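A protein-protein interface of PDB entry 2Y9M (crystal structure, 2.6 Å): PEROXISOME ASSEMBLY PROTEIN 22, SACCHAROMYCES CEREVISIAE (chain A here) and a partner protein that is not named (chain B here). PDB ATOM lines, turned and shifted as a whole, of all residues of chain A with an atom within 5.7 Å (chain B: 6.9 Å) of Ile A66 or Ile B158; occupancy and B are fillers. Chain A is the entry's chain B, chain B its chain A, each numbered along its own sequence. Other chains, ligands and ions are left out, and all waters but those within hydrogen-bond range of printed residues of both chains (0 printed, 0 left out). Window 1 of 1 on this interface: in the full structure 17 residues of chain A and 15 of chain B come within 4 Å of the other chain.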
ATOM      1  N   VAL A  36      19.533 -18.835 -30.607  1.00  0.00           N
ATOM      2  CA  VAL A  36      18.116 -18.956 -30.381  1.00  0.00           C
ATOM      3  C   VAL A  36      17.611 -20.005 -31.318  1.00  0.00           C
ATOM      4  O   VAL A  36      18.042 -20.057 -32.473  1.00  0.00           O
ATOM      5  CB  VAL A  36      17.383 -17.627 -30.591  1.00  0.00           C
ATOM      6  CG1 VAL A  36      15.857 -17.792 -30.375  1.00  0.00           C
ATOM      7  CG2 VAL A  36      17.919 -16.638 -29.611  1.00  0.00           C
ATOM      8  N   LEU A  37      16.729 -20.873 -30.818  1.00  0.00           N
ATOM      9  CA  LEU A  37      16.170 -21.963 -31.638  1.00  0.00           C
ATOM     10  C   LEU A  37      14.691 -21.689 -31.875  1.00  0.00           C
ATOM     11  O   LEU A  37      13.887 -21.624 -30.929  1.00  0.00           O
ATOM     12  CB  LEU A  37      16.407 -23.327 -30.983  1.00  0.00           C
ATOM     13  CG  LEU A  37      17.720 -24.040 -31.346  1.00  0.00           C
ATOM     14  CD1 LEU A  37      18.953 -23.291 -30.825  1.00  0.00           C
ATOM     15  CD2 LEU A  37      17.763 -25.493 -30.834  1.00  0.00           C
ATOM     16  N   LEU A  38      14.337 -21.444 -33.125  1.00  0.00           N
ATOM     17  CA  LEU A  38      12.958 -21.143 -33.457  1.00  0.00           C
ATOM     18  C   LEU A  38      12.340 -22.389 -34.073  1.00  0.00           C
ATOM     19  O   LEU A  38      12.736 -22.803 -35.169  1.00  0.00           O
ATOM     20  CB  LEU A  38      12.864 -19.966 -34.431  1.00  0.00           C
ATOM     21  CG  LEU A  38      13.425 -18.602 -33.998  1.00  0.00           C
ATOM     22  CD1 LEU A  38      12.987 -17.490 -34.951  1.00  0.00           C
ATOM     23  CD2 LEU A  38      13.016 -18.256 -32.620  1.00  0.00           C
ATOM     24  N   VAL A  39      11.385 -22.989 -33.363  1.00  0.00           N
ATOM     25  CA  VAL A  39      10.749 -24.215 -33.813  1.00  0.00           C
ATOM     26  C   VAL A  39       9.427 -23.883 -34.513  1.00  0.00           C
ATOM     27  O   VAL A  39       8.511 -23.346 -33.879  1.00  0.00           O
ATOM     28  CB  VAL A  39      10.443 -25.186 -32.622  1.00  0.00           C
ATOM     29  CG1 VAL A  39       9.961 -26.532 -33.147  1.00  0.00           C
ATOM     30  CG2 VAL A  39      11.649 -25.369 -31.719  1.00  0.00           C
ATOM     31  N   PRO A  40       9.322 -24.194 -35.818  1.00  0.00           N
ATOM     32  CA  PRO A  40       8.066 -23.982 -36.523  1.00  0.00           C
ATOM     33  C   PRO A  40       7.096 -25.129 -36.314  1.00  0.00           C
ATOM     34  O   PRO A  40       7.138 -26.110 -37.060  1.00  0.00           O
ATOM     35  CB  PRO A  40       8.494 -23.907 -37.996  1.00  0.00           C
ATOM     36  CG  PRO A  40       9.835 -24.518 -38.075  1.00  0.00           C
ATOM     37  CD  PRO A  40      10.363 -24.767 -36.691  1.00  0.00           C
ATOM     38  N   GLU A  62      17.030 -23.249 -21.411  1.00  0.00           N
ATOM     39  CA  GLU A  62      15.786 -23.696 -22.017  1.00  0.00           C
ATOM     40  C   GLU A  62      15.012 -22.539 -22.647  1.00  0.00           C
ATOM     41  O   GLU A  62      14.305 -22.731 -23.638  1.00  0.00           O
ATOM     42  CB  GLU A  62      14.919 -24.437 -21.004  1.00  0.00           C
ATOM     43  CG  GLU A  62      13.720 -25.089 -21.662  1.00  0.00           C
ATOM     44  CD  GLU A  62      12.954 -26.010 -20.730  1.00  0.00           C
ATOM     45  OE1 GLU A  62      13.149 -25.877 -19.497  1.00  0.00           O
ATOM     46  OE2 GLU A  62      12.164 -26.853 -21.234  1.00  0.00           O
ATOM     47  N   HIS A  63      15.158 -21.347 -22.081  1.00  0.00           N
ATOM     48  CA  HIS A  63      14.537 -20.145 -22.637  1.00  0.00           C
ATOM     49  C   HIS A  63      14.981 -19.809 -24.070  1.00  0.00           C
ATOM     50  O   HIS A  63      14.326 -19.013 -24.719  1.00  0.00           O
ATOM     51  CB  HIS A  63      14.779 -18.941 -21.721  1.00  0.00           C
ATOM     52  CG  HIS A  63      16.219 -18.539 -21.613  1.00  0.00           C
ATOM     53  ND1 HIS A  63      17.099 -19.145 -20.742  1.00  0.00           N
ATOM     54  CD2 HIS A  63      16.923 -17.567 -22.239  1.00  0.00           C
ATOM     55  CE1 HIS A  63      18.286 -18.578 -20.849  1.00  0.00           C
ATOM     56  NE2 HIS A  63      18.206 -17.614 -21.748  1.00  0.00           N
ATOM     57  N   LYS A  64      16.056 -20.428 -24.561  1.00  0.00           N
ATOM     58  CA  LYS A  64      16.525 -20.218 -25.952  1.00  0.00           C
ATOM     59  C   LYS A  64      15.777 -21.036 -27.005  1.00  0.00           C
ATOM     60  O   LYS A  64      15.973 -20.875 -28.228  1.00  0.00           O
ATOM     61  CB  LYS A  64      18.025 -20.455 -26.071  1.00  0.00           C
ATOM     62  CG  LYS A  64      18.866 -19.401 -25.350  1.00  0.00           C
ATOM     63  CD  LYS A  64      20.264 -19.927 -25.065  1.00  0.00           C
ATOM     64  CE  LYS A  64      20.994 -19.073 -24.033  1.00  0.00           C
ATOM     65  NZ  LYS A  64      22.460 -19.409 -23.970  1.00  0.00           N
ATOM     66  N   ILE A  65      14.889 -21.903 -26.543  1.00  0.00           N
ATOM     67  CA  ILE A  65      14.015 -22.610 -27.471  1.00  0.00           C
ATOM     68  C   ILE A  65      12.672 -21.894 -27.543  1.00  0.00           C
ATOM     69  O   ILE A  65      12.016 -21.667 -26.526  1.00  0.00           O
ATOM     70  CB  ILE A  65      13.877 -24.122 -27.125  1.00  0.00           C
ATOM     71  CG1 ILE A  65      15.272 -24.763 -27.094  1.00  0.00           C
ATOM     72  CG2 ILE A  65      12.998 -24.817 -28.148  1.00  0.00           C
ATOM     73  CD1 ILE A  65      15.349 -26.219 -26.585  1.00  0.00           C
ATOM     74  N   ILE A  66      12.269 -21.503 -28.745  1.00  0.00           N
ATOM     75  CA  ILE A  66      11.001 -20.805 -28.877  1.00  0.00           C
ATOM     76  C   ILE A  66      10.118 -21.496 -29.891  1.00  0.00           C
ATOM     77  O   ILE A  66      10.518 -21.707 -31.041  1.00  0.00           O
ATOM     78  CB  ILE A  66      11.189 -19.340 -29.271  1.00  0.00           C
ATOM     79  CG1 ILE A  66      11.906 -18.572 -28.164  1.00  0.00           C
ATOM     80  CG2 ILE A  66       9.838 -18.686 -29.524  1.00  0.00           C
ATOM     81  CD1 ILE A  66      12.344 -17.145 -28.625  1.00  0.00           C
ATOM     82  N   TYR A  67       8.912 -21.852 -29.458  1.00  0.00           N
ATOM     83  CA  TYR A  67       7.965 -22.544 -30.325  1.00  0.00           C
ATOM     84  C   TYR A  67       7.094 -21.514 -31.014  1.00  0.00           C
ATOM     85  O   TYR A  67       6.605 -20.599 -30.371  1.00  0.00           O
ATOM     86  CB  TYR A  67       7.132 -23.547 -29.526  1.00  0.00           C
ATOM     87  CG  TYR A  67       7.924 -24.771 -29.132  1.00  0.00           C
ATOM     88  CD1 TYR A  67       7.992 -25.889 -29.967  1.00  0.00           C
ATOM     89  CD2 TYR A  67       8.623 -24.808 -27.934  1.00  0.00           C
ATOM     90  CE1 TYR A  67       8.725 -27.021 -29.609  1.00  0.00           C
ATOM     91  CE2 TYR A  67       9.357 -25.934 -27.563  1.00  0.00           C
ATOM     92  CZ  TYR A  67       9.406 -27.030 -28.404  1.00  0.00           C
ATOM     93  OH  TYR A  67      10.160 -28.115 -28.024  1.00  0.00           O
ATOM     94  N   CYS A  68       6.920 -21.663 -32.322  1.00  0.00           N
ATOM     95  CA  CYS A  68       6.237 -20.679 -33.120  1.00  0.00           C
ATOM     96  C   CYS A  68       5.061 -21.307 -33.835  1.00  0.00           C
ATOM     97  O   CYS A  68       5.242 -22.181 -34.701  1.00  0.00           O
ATOM     98  CB  CYS A  68       7.189 -20.116 -34.156  1.00  0.00           C
ATOM     99  SG  CYS A  68       8.573 -19.200 -33.412  1.00  0.00           S
ATOM    100  N   SER A  76       8.837 -12.668 -37.545  1.00  0.00           N
ATOM    101  CA  SER A  76       8.849 -11.517 -36.666  1.00  0.00           C
ATOM    102  C   SER A  76       9.853 -11.705 -35.536  1.00  0.00           C
ATOM    103  O   SER A  76      10.520 -10.754 -35.149  1.00  0.00           O
ATOM    104  CB  SER A  76       7.465 -11.200 -36.136  1.00  0.00           C
ATOM    105  OG  SER A  76       6.808 -10.358 -37.059  1.00  0.00           O
ATOM    106  N   CYS A  77       9.996 -12.919 -35.023  1.00  0.00           N
ATOM    107  CA  CYS A  77      11.029 -13.193 -34.026  1.00  0.00           C
ATOM    108  C   CYS A  77      12.441 -12.965 -34.607  1.00  0.00           C
ATOM    109  O   CYS A  77      13.282 -12.276 -33.979  1.00  0.00           O
ATOM    110  CB  CYS A  77      10.888 -14.608 -33.489  1.00  0.00           C
ATOM    111  SG  CYS A  77       9.578 -14.788 -32.284  1.00  0.00           S
ATOM    112  N   ARG A  80      13.237  -9.245 -34.725  1.00  0.00           N
ATOM    113  CA  ARG A  80      13.371  -8.582 -33.467  1.00  0.00           C
ATOM    114  C   ARG A  80      14.616  -8.939 -32.691  1.00  0.00           C
ATOM    115  O   ARG A  80      15.071  -8.171 -31.829  1.00  0.00           O
ATOM    116  CB  ARG A  80      12.157  -8.895 -32.595  1.00  0.00           C
ATOM    117  CG  ARG A  80      12.011  -7.922 -31.421  1.00  0.00           C
ATOM    118  CD  ARG A  80      11.497  -6.602 -31.925  1.00  0.00           C
ATOM    119  NE  ARG A  80      11.883  -5.445 -31.112  1.00  0.00           N
ATOM    120  CZ  ARG A  80      13.005  -4.739 -31.283  1.00  0.00           C
ATOM    121  NH1 ARG A  80      13.880  -5.093 -32.209  1.00  0.00           N
ATOM    122  NH2 ARG A  80      13.261  -3.691 -30.511  1.00  0.00           N
ATOM    123  N   LEU A  81      15.134 -10.130 -32.912  1.00  0.00           N
ATOM    124  CA  LEU A  81      16.257 -10.593 -32.124  1.00  0.00           C
ATOM    125  C   LEU A  81      17.520 -10.074 -32.825  1.00  0.00           C
ATOM    126  O   LEU A  81      18.450  -9.647 -32.168  1.00  0.00           O
ATOM    127  CB  LEU A  81      16.235 -12.120 -32.019  1.00  0.00           C
ATOM    128  CG  LEU A  81      15.017 -12.769 -31.348  1.00  0.00           C
ATOM    129  CD1 LEU A  81      14.968 -14.264 -31.637  1.00  0.00           C
ATOM    130  CD2 LEU A  81      15.041 -12.558 -29.848  1.00  0.00           C
ATOM    131  N   PRO B  61       3.756 -13.123 -19.742  1.00  0.00           N
ATOM    132  CA  PRO B  61       5.167 -13.473 -19.795  1.00  0.00           C
ATOM    133  C   PRO B  61       6.092 -12.499 -19.025  1.00  0.00           C
ATOM    134  O   PRO B  61       7.310 -12.731 -18.961  1.00  0.00           O
ATOM    135  CB  PRO B  61       5.459 -13.472 -21.295  1.00  0.00           C
ATOM    136  CG  PRO B  61       4.374 -12.671 -21.899  1.00  0.00           C
ATOM    137  CD  PRO B  61       3.179 -12.974 -21.087  1.00  0.00           C
ATOM    138  N   LEU B  92      10.013  -5.887 -23.737  1.00  0.00           N
ATOM    139  CA  LEU B  92       9.544  -5.951 -25.111  1.00  0.00           C
ATOM    140  C   LEU B  92       8.029  -6.021 -25.051  1.00  0.00           C
ATOM    141  O   LEU B  92       7.486  -7.013 -24.563  1.00  0.00           O
ATOM    142  CB  LEU B  92      10.014  -7.227 -25.804  1.00  0.00           C
ATOM    143  CG  LEU B  92      11.424  -7.460 -26.278  1.00  0.00           C
ATOM    144  CD1 LEU B  92      11.467  -8.853 -26.881  1.00  0.00           C
ATOM    145  CD2 LEU B  92      11.771  -6.425 -27.311  1.00  0.00           C
ATOM    146  N   ILE B 143       6.715  -7.015 -32.510  1.00  0.00           N
ATOM    147  CA  ILE B 143       5.961  -7.648 -31.428  1.00  0.00           C
ATOM    148  C   ILE B 143       4.473  -7.489 -31.722  1.00  0.00           C
ATOM    149  O   ILE B 143       3.701  -8.396 -31.483  1.00  0.00           O
ATOM    150  CB  ILE B 143       6.300  -7.077 -30.013  1.00  0.00           C
ATOM    151  CG1 ILE B 143       7.761  -7.329 -29.686  1.00  0.00           C
ATOM    152  CG2 ILE B 143       5.399  -7.710 -28.945  1.00  0.00           C
ATOM    153  CD1 ILE B 143       8.111  -8.794 -29.568  1.00  0.00           C
ATOM    154  N   ILE B 146       3.301 -10.265 -34.225  1.00  0.00           N
ATOM    155  CA  ILE B 146       3.179 -11.584 -33.633  1.00  0.00           C
ATOM    156  C   ILE B 146       1.757 -11.724 -33.079  1.00  0.00           C
ATOM    157  O   ILE B 146       0.970 -12.533 -33.574  1.00  0.00           O
ATOM    158  CB  ILE B 146       4.231 -11.816 -32.518  1.00  0.00           C
ATOM    159  CG1 ILE B 146       5.649 -11.751 -33.080  1.00  0.00           C
ATOM    160  CG2 ILE B 146       4.024 -13.177 -31.858  1.00  0.00           C
ATOM    161  CD1 ILE B 146       6.741 -11.956 -32.008  1.00  0.00           C
ATOM    162  N   SER B 153       2.479 -18.741 -28.873  1.00  0.00           N
ATOM    163  CA  SER B 153       3.700 -19.456 -28.496  1.00  0.00           C
ATOM    164  C   SER B 153       4.930 -18.587 -28.748  1.00  0.00           C
ATOM    165  O   SER B 153       5.807 -18.529 -27.908  1.00  0.00           O
ATOM    166  CB  SER B 153       3.829 -20.794 -29.230  1.00  0.00           C
ATOM    167  OG  SER B 153       2.792 -21.685 -28.875  1.00  0.00           O
ATOM    168  N   ALA B 154       4.985 -17.910 -29.887  1.00  0.00           N
ATOM    169  CA  ALA B 154       6.102 -17.036 -30.176  1.00  0.00           C
ATOM    170  C   ALA B 154       6.121 -15.799 -29.255  1.00  0.00           C
ATOM    171  O   ALA B 154       7.190 -15.345 -28.808  1.00  0.00           O
ATOM    172  CB  ALA B 154       6.092 -16.629 -31.662  1.00  0.00           C
ATOM    173  N   TYR B 155       4.936 -15.252 -28.977  1.00  0.00           N
ATOM    174  CA  TYR B 155       4.819 -14.109 -28.063  1.00  0.00           C
ATOM    175  C   TYR B 155       5.347 -14.415 -26.668  1.00  0.00           C
ATOM    176  O   TYR B 155       6.108 -13.616 -26.119  1.00  0.00           O
ATOM    177  CB  TYR B 155       3.383 -13.616 -27.958  1.00  0.00           C
ATOM    178  CG  TYR B 155       3.192 -12.496 -26.966  1.00  0.00           C
ATOM    179  CD1 TYR B 155       3.947 -11.339 -27.053  1.00  0.00           C
ATOM    180  CD2 TYR B 155       2.254 -12.592 -25.946  1.00  0.00           C
ATOM    181  CE1 TYR B 155       3.775 -10.299 -26.172  1.00  0.00           C
ATOM    182  CE2 TYR B 155       2.070 -11.555 -25.041  1.00  0.00           C
ATOM    183  CZ  TYR B 155       2.840 -10.402 -25.162  1.00  0.00           C
ATOM    184  OH  TYR B 155       2.679  -9.351 -24.276  1.00  0.00           O
ATOM    185  N   GLN B 156       4.971 -15.555 -26.093  1.00  0.00           N
ATOM    186  CA  GLN B 156       5.437 -15.894 -24.750  1.00  0.00           C
ATOM    187  C   GLN B 156       6.916 -16.303 -24.753  1.00  0.00           C
ATOM    188  O   GLN B 156       7.652 -16.045 -23.801  1.00  0.00           O
ATOM    189  CB  GLN B 156       4.557 -16.985 -24.096  1.00  0.00           C
ATOM    190  CG  GLN B 156       3.028 -16.752 -24.234  1.00  0.00           C
ATOM    191  CD  GLN B 156       2.278 -16.827 -22.916  1.00  0.00           C
ATOM    192  OE1 GLN B 156       2.623 -17.624 -22.030  1.00  0.00           O
ATOM    193  NE2 GLN B 156       1.239 -15.995 -22.776  1.00  0.00           N
ATOM    194  N   GLY B 157       7.344 -16.941 -25.831  1.00  0.00           N
ATOM    195  CA  GLY B 157       8.727 -17.380 -25.950  1.00  0.00           C
ATOM    196  C   GLY B 157       9.721 -16.237 -26.086  1.00  0.00           C
ATOM    197  O   GLY B 157      10.713 -16.176 -25.356  1.00  0.00           O
ATOM    198  N   ILE B 158       9.468 -15.331 -27.029  1.00  0.00           N
ATOM    199  CA  ILE B 158      10.316 -14.163 -27.203  1.00  0.00           C
ATOM    200  C   ILE B 158      10.404 -13.258 -25.973  1.00  0.00           C
ATOM    201  O   ILE B 158      11.488 -12.771 -25.626  1.00  0.00           O
ATOM    202  CB  ILE B 158       9.949 -13.373 -28.442  1.00  0.00           C
ATOM    203  CG1 ILE B 158      11.184 -12.641 -28.926  1.00  0.00           C
ATOM    204  CG2 ILE B 158       8.809 -12.424 -28.179  1.00  0.00           C
ATOM    205  CD1 ILE B 158      11.118 -12.308 -30.335  1.00  0.00           C
ATOM    206  N   VAL B 159       9.286 -13.055 -25.287  1.00  0.00           N
ATOM    207  CA  VAL B 159       9.313 -12.222 -24.096  1.00  0.00           C
ATOM    208  C   VAL B 159      10.124 -12.890 -22.980  1.00  0.00           C
ATOM    209  O   VAL B 159      10.896 -12.227 -22.273  1.00  0.00           O
ATOM    210  CB  VAL B 159       7.884 -11.817 -23.638  1.00  0.00           C
ATOM    211  CG1 VAL B 159       7.908 -11.129 -22.274  1.00  0.00           C
ATOM    212  CG2 VAL B 159       7.242 -10.916 -24.691  1.00  0.00           C
ATOM    213  N   LYS B 160       9.964 -14.202 -22.835  1.00  0.00           N
ATOM    214  CA  LYS B 160      10.675 -14.945 -21.785  1.00  0.00           C
ATOM    215  C   LYS B 160      12.141 -15.054 -22.143  1.00  0.00           C
ATOM    216  O   LYS B 160      13.020 -14.901 -21.280  1.00  0.00           O
ATOM    217  CB  LYS B 160      10.051 -16.322 -21.542  1.00  0.00           C
ATOM    218  CG  LYS B 160       8.727 -16.252 -20.748  1.00  0.00           C
ATOM    219  CD  LYS B 160       7.930 -17.562 -20.817  1.00  0.00           C
ATOM    220  CE  LYS B 160       6.428 -17.297 -20.783  1.00  0.00           C
ATOM    221  NZ  LYS B 160       5.583 -18.558 -20.842  1.00  0.00           N
ATOM    222  N   TYR B 161      12.407 -15.283 -23.423  1.00  0.00           N
ATOM    223  CA  TYR B 161      13.765 -15.247 -23.896  1.00  0.00           C
ATOM    224  C   TYR B 161      14.379 -13.902 -23.493  1.00  0.00           C
ATOM    225  O   TYR B 161      15.407 -13.848 -22.799  1.00  0.00           O
ATOM    226  CB  TYR B 161      13.853 -15.434 -25.409  1.00  0.00           C
ATOM    227  CG  TYR B 161      15.265 -15.208 -25.914  1.00  0.00           C
ATOM    228  CD1 TYR B 161      16.216 -16.224 -25.856  1.00  0.00           C
ATOM    229  CD2 TYR B 161      15.664 -13.970 -26.383  1.00  0.00           C
ATOM    230  CE1 TYR B 161      17.517 -16.009 -26.280  1.00  0.00           C
ATOM    231  CE2 TYR B 161      16.957 -13.739 -26.818  1.00  0.00           C
ATOM    232  CZ  TYR B 161      17.884 -14.752 -26.774  1.00  0.00           C
ATOM    233  OH  TYR B 161      19.176 -14.517 -27.226  1.00  0.00           O
ATOM    234  N   PHE B 162      13.721 -12.817 -23.887  1.00  0.00           N
ATOM    235  CA  PHE B 162      14.266 -11.502 -23.624  1.00  0.00           C
ATOM    236  C   PHE B 162      14.515 -11.247 -22.126  1.00  0.00           C
ATOM    237  O   PHE B 162      15.569 -10.733 -21.744  1.00  0.00           O
ATOM    238  CB  PHE B 162      13.387 -10.408 -24.241  1.00  0.00           C
ATOM    239  CG  PHE B 162      13.933  -9.024 -24.029  1.00  0.00           C
ATOM    240  CD1 PHE B 162      13.627  -8.310 -22.873  1.00  0.00           C
ATOM    241  CD2 PHE B 162      14.761  -8.446 -24.974  1.00  0.00           C
ATOM    242  CE1 PHE B 162      14.147  -7.046 -22.664  1.00  0.00           C
ATOM    243  CE2 PHE B 162      15.289  -7.178 -24.768  1.00  0.00           C
ATOM    244  CZ  PHE B 162      14.975  -6.479 -23.608  1.00  0.00           C
ATOM    245  N   LEU B 163      13.547 -11.601 -21.285  1.00  0.00           N
ATOM    246  CA  LEU B 163      13.651 -11.292 -19.843  1.00  0.00           C
ATOM    247  C   LEU B 163      14.707 -12.115 -19.128  1.00  0.00           C
ATOM    248  O   LEU B 163      15.358 -11.614 -18.217  1.00  0.00           O
ATOM    249  CB  LEU B 163      12.308 -11.445 -19.121  1.00  0.00           C
ATOM    250  CG  LEU B 163      11.271 -10.424 -19.568  1.00  0.00           C
ATOM    251  CD1 LEU B 163       9.914 -10.749 -18.999  1.00  0.00           C
ATOM    252  CD2 LEU B 163      11.721  -9.020 -19.167  1.00  0.00           C
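Among the printed residues, pairs that only touch across the chains: Val A36 with Tyr B161 (3.4 Å), Cys A77 with Ile B158 (3.5 Å), His A63 with Tyr B161 (3.6 Å), Ser A76 with Ile B146 (3.6 Å), Ile A66 with Ile B158 (3.8 Å), Ile A66 with Gly B157 (3.8 Å), Lys A64 with Tyr B161 (3.8 Å), Leu A81 with Tyr B161 (3.8 Å), Arg A80 with Leu B92 (3.9 Å), Ile A66 with Tyr B161 (3.9 Å), Leu A81 with Ile B158 (3.96 Å), Cys A68 with Ala B154 (3.98 Å) and Cys A77 with Ala B154 (3.99 Å).
Leu A37 touches none of the printed residues of chain B.
Leu A38 touches none of the printed residues of chain B.
Of the printed residues of chain B, Lys A64 touches Tyr B161 (3.8 Å).
Of chain B, only Gly B157, Ile B158 and Tyr B161 come within 4 Å of Ile A66.
Printed residues of chain A within 4 Å of Ser B153: Tyr A67.
Of the printed residues of chain A, Gly B157 touches Ile A66 (3.8 Å).
Ile B158 touches just these residues of chain A: Ile A66, Cys A77 and Leu A81.
The nearest residue of chain B that does not touch Ile A66 is Ala B154 (4.1 Å).
The nearest residue of chain A that does not touch Ile B158 is Arg A80 (4.2 Å).
The nearest printed residue of chain A that does not touch Ile B146 is Cys A77 (4.02 Å).
N of Ala B154 is in hydrogen-bond range of O of Tyr A67.
O of Ser B153 lies close to O of Tyr A67 (3.3 Å).
Printed residues of chain B that touch a printed residue of chain A: Leu B92, Ile B146, Ser B153, Ala B154, Gly B157, Ile B158 and Tyr B161.
Hydrophobic or aromatic side chains of chain B within 4 Å of the printed part of chain A: Leu B92, Ile B146, Ala B154, Ile B158 and Tyr B161.
The backbone NH (N) of Val A39 lies within hydrogen-bond range of the backbone carbonyl oxygen (O) of Ile A66 (2.8 Å).
The backbone carbonyl oxygen (O) of Val A39 lies within hydrogen-bond range of the backbone NH (N) of Cys A68 (2.8 Å).
The backbone carbonyl oxygen of Leu A37 sits at hydrogen-bond distance from the backbone NH of Ile A66 (2.7 Å).
The backbone NH (N) of Leu A37 lies within hydrogen-bond range of the backbone carbonyl oxygen (O) of Lys A64 (2.7 Å).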
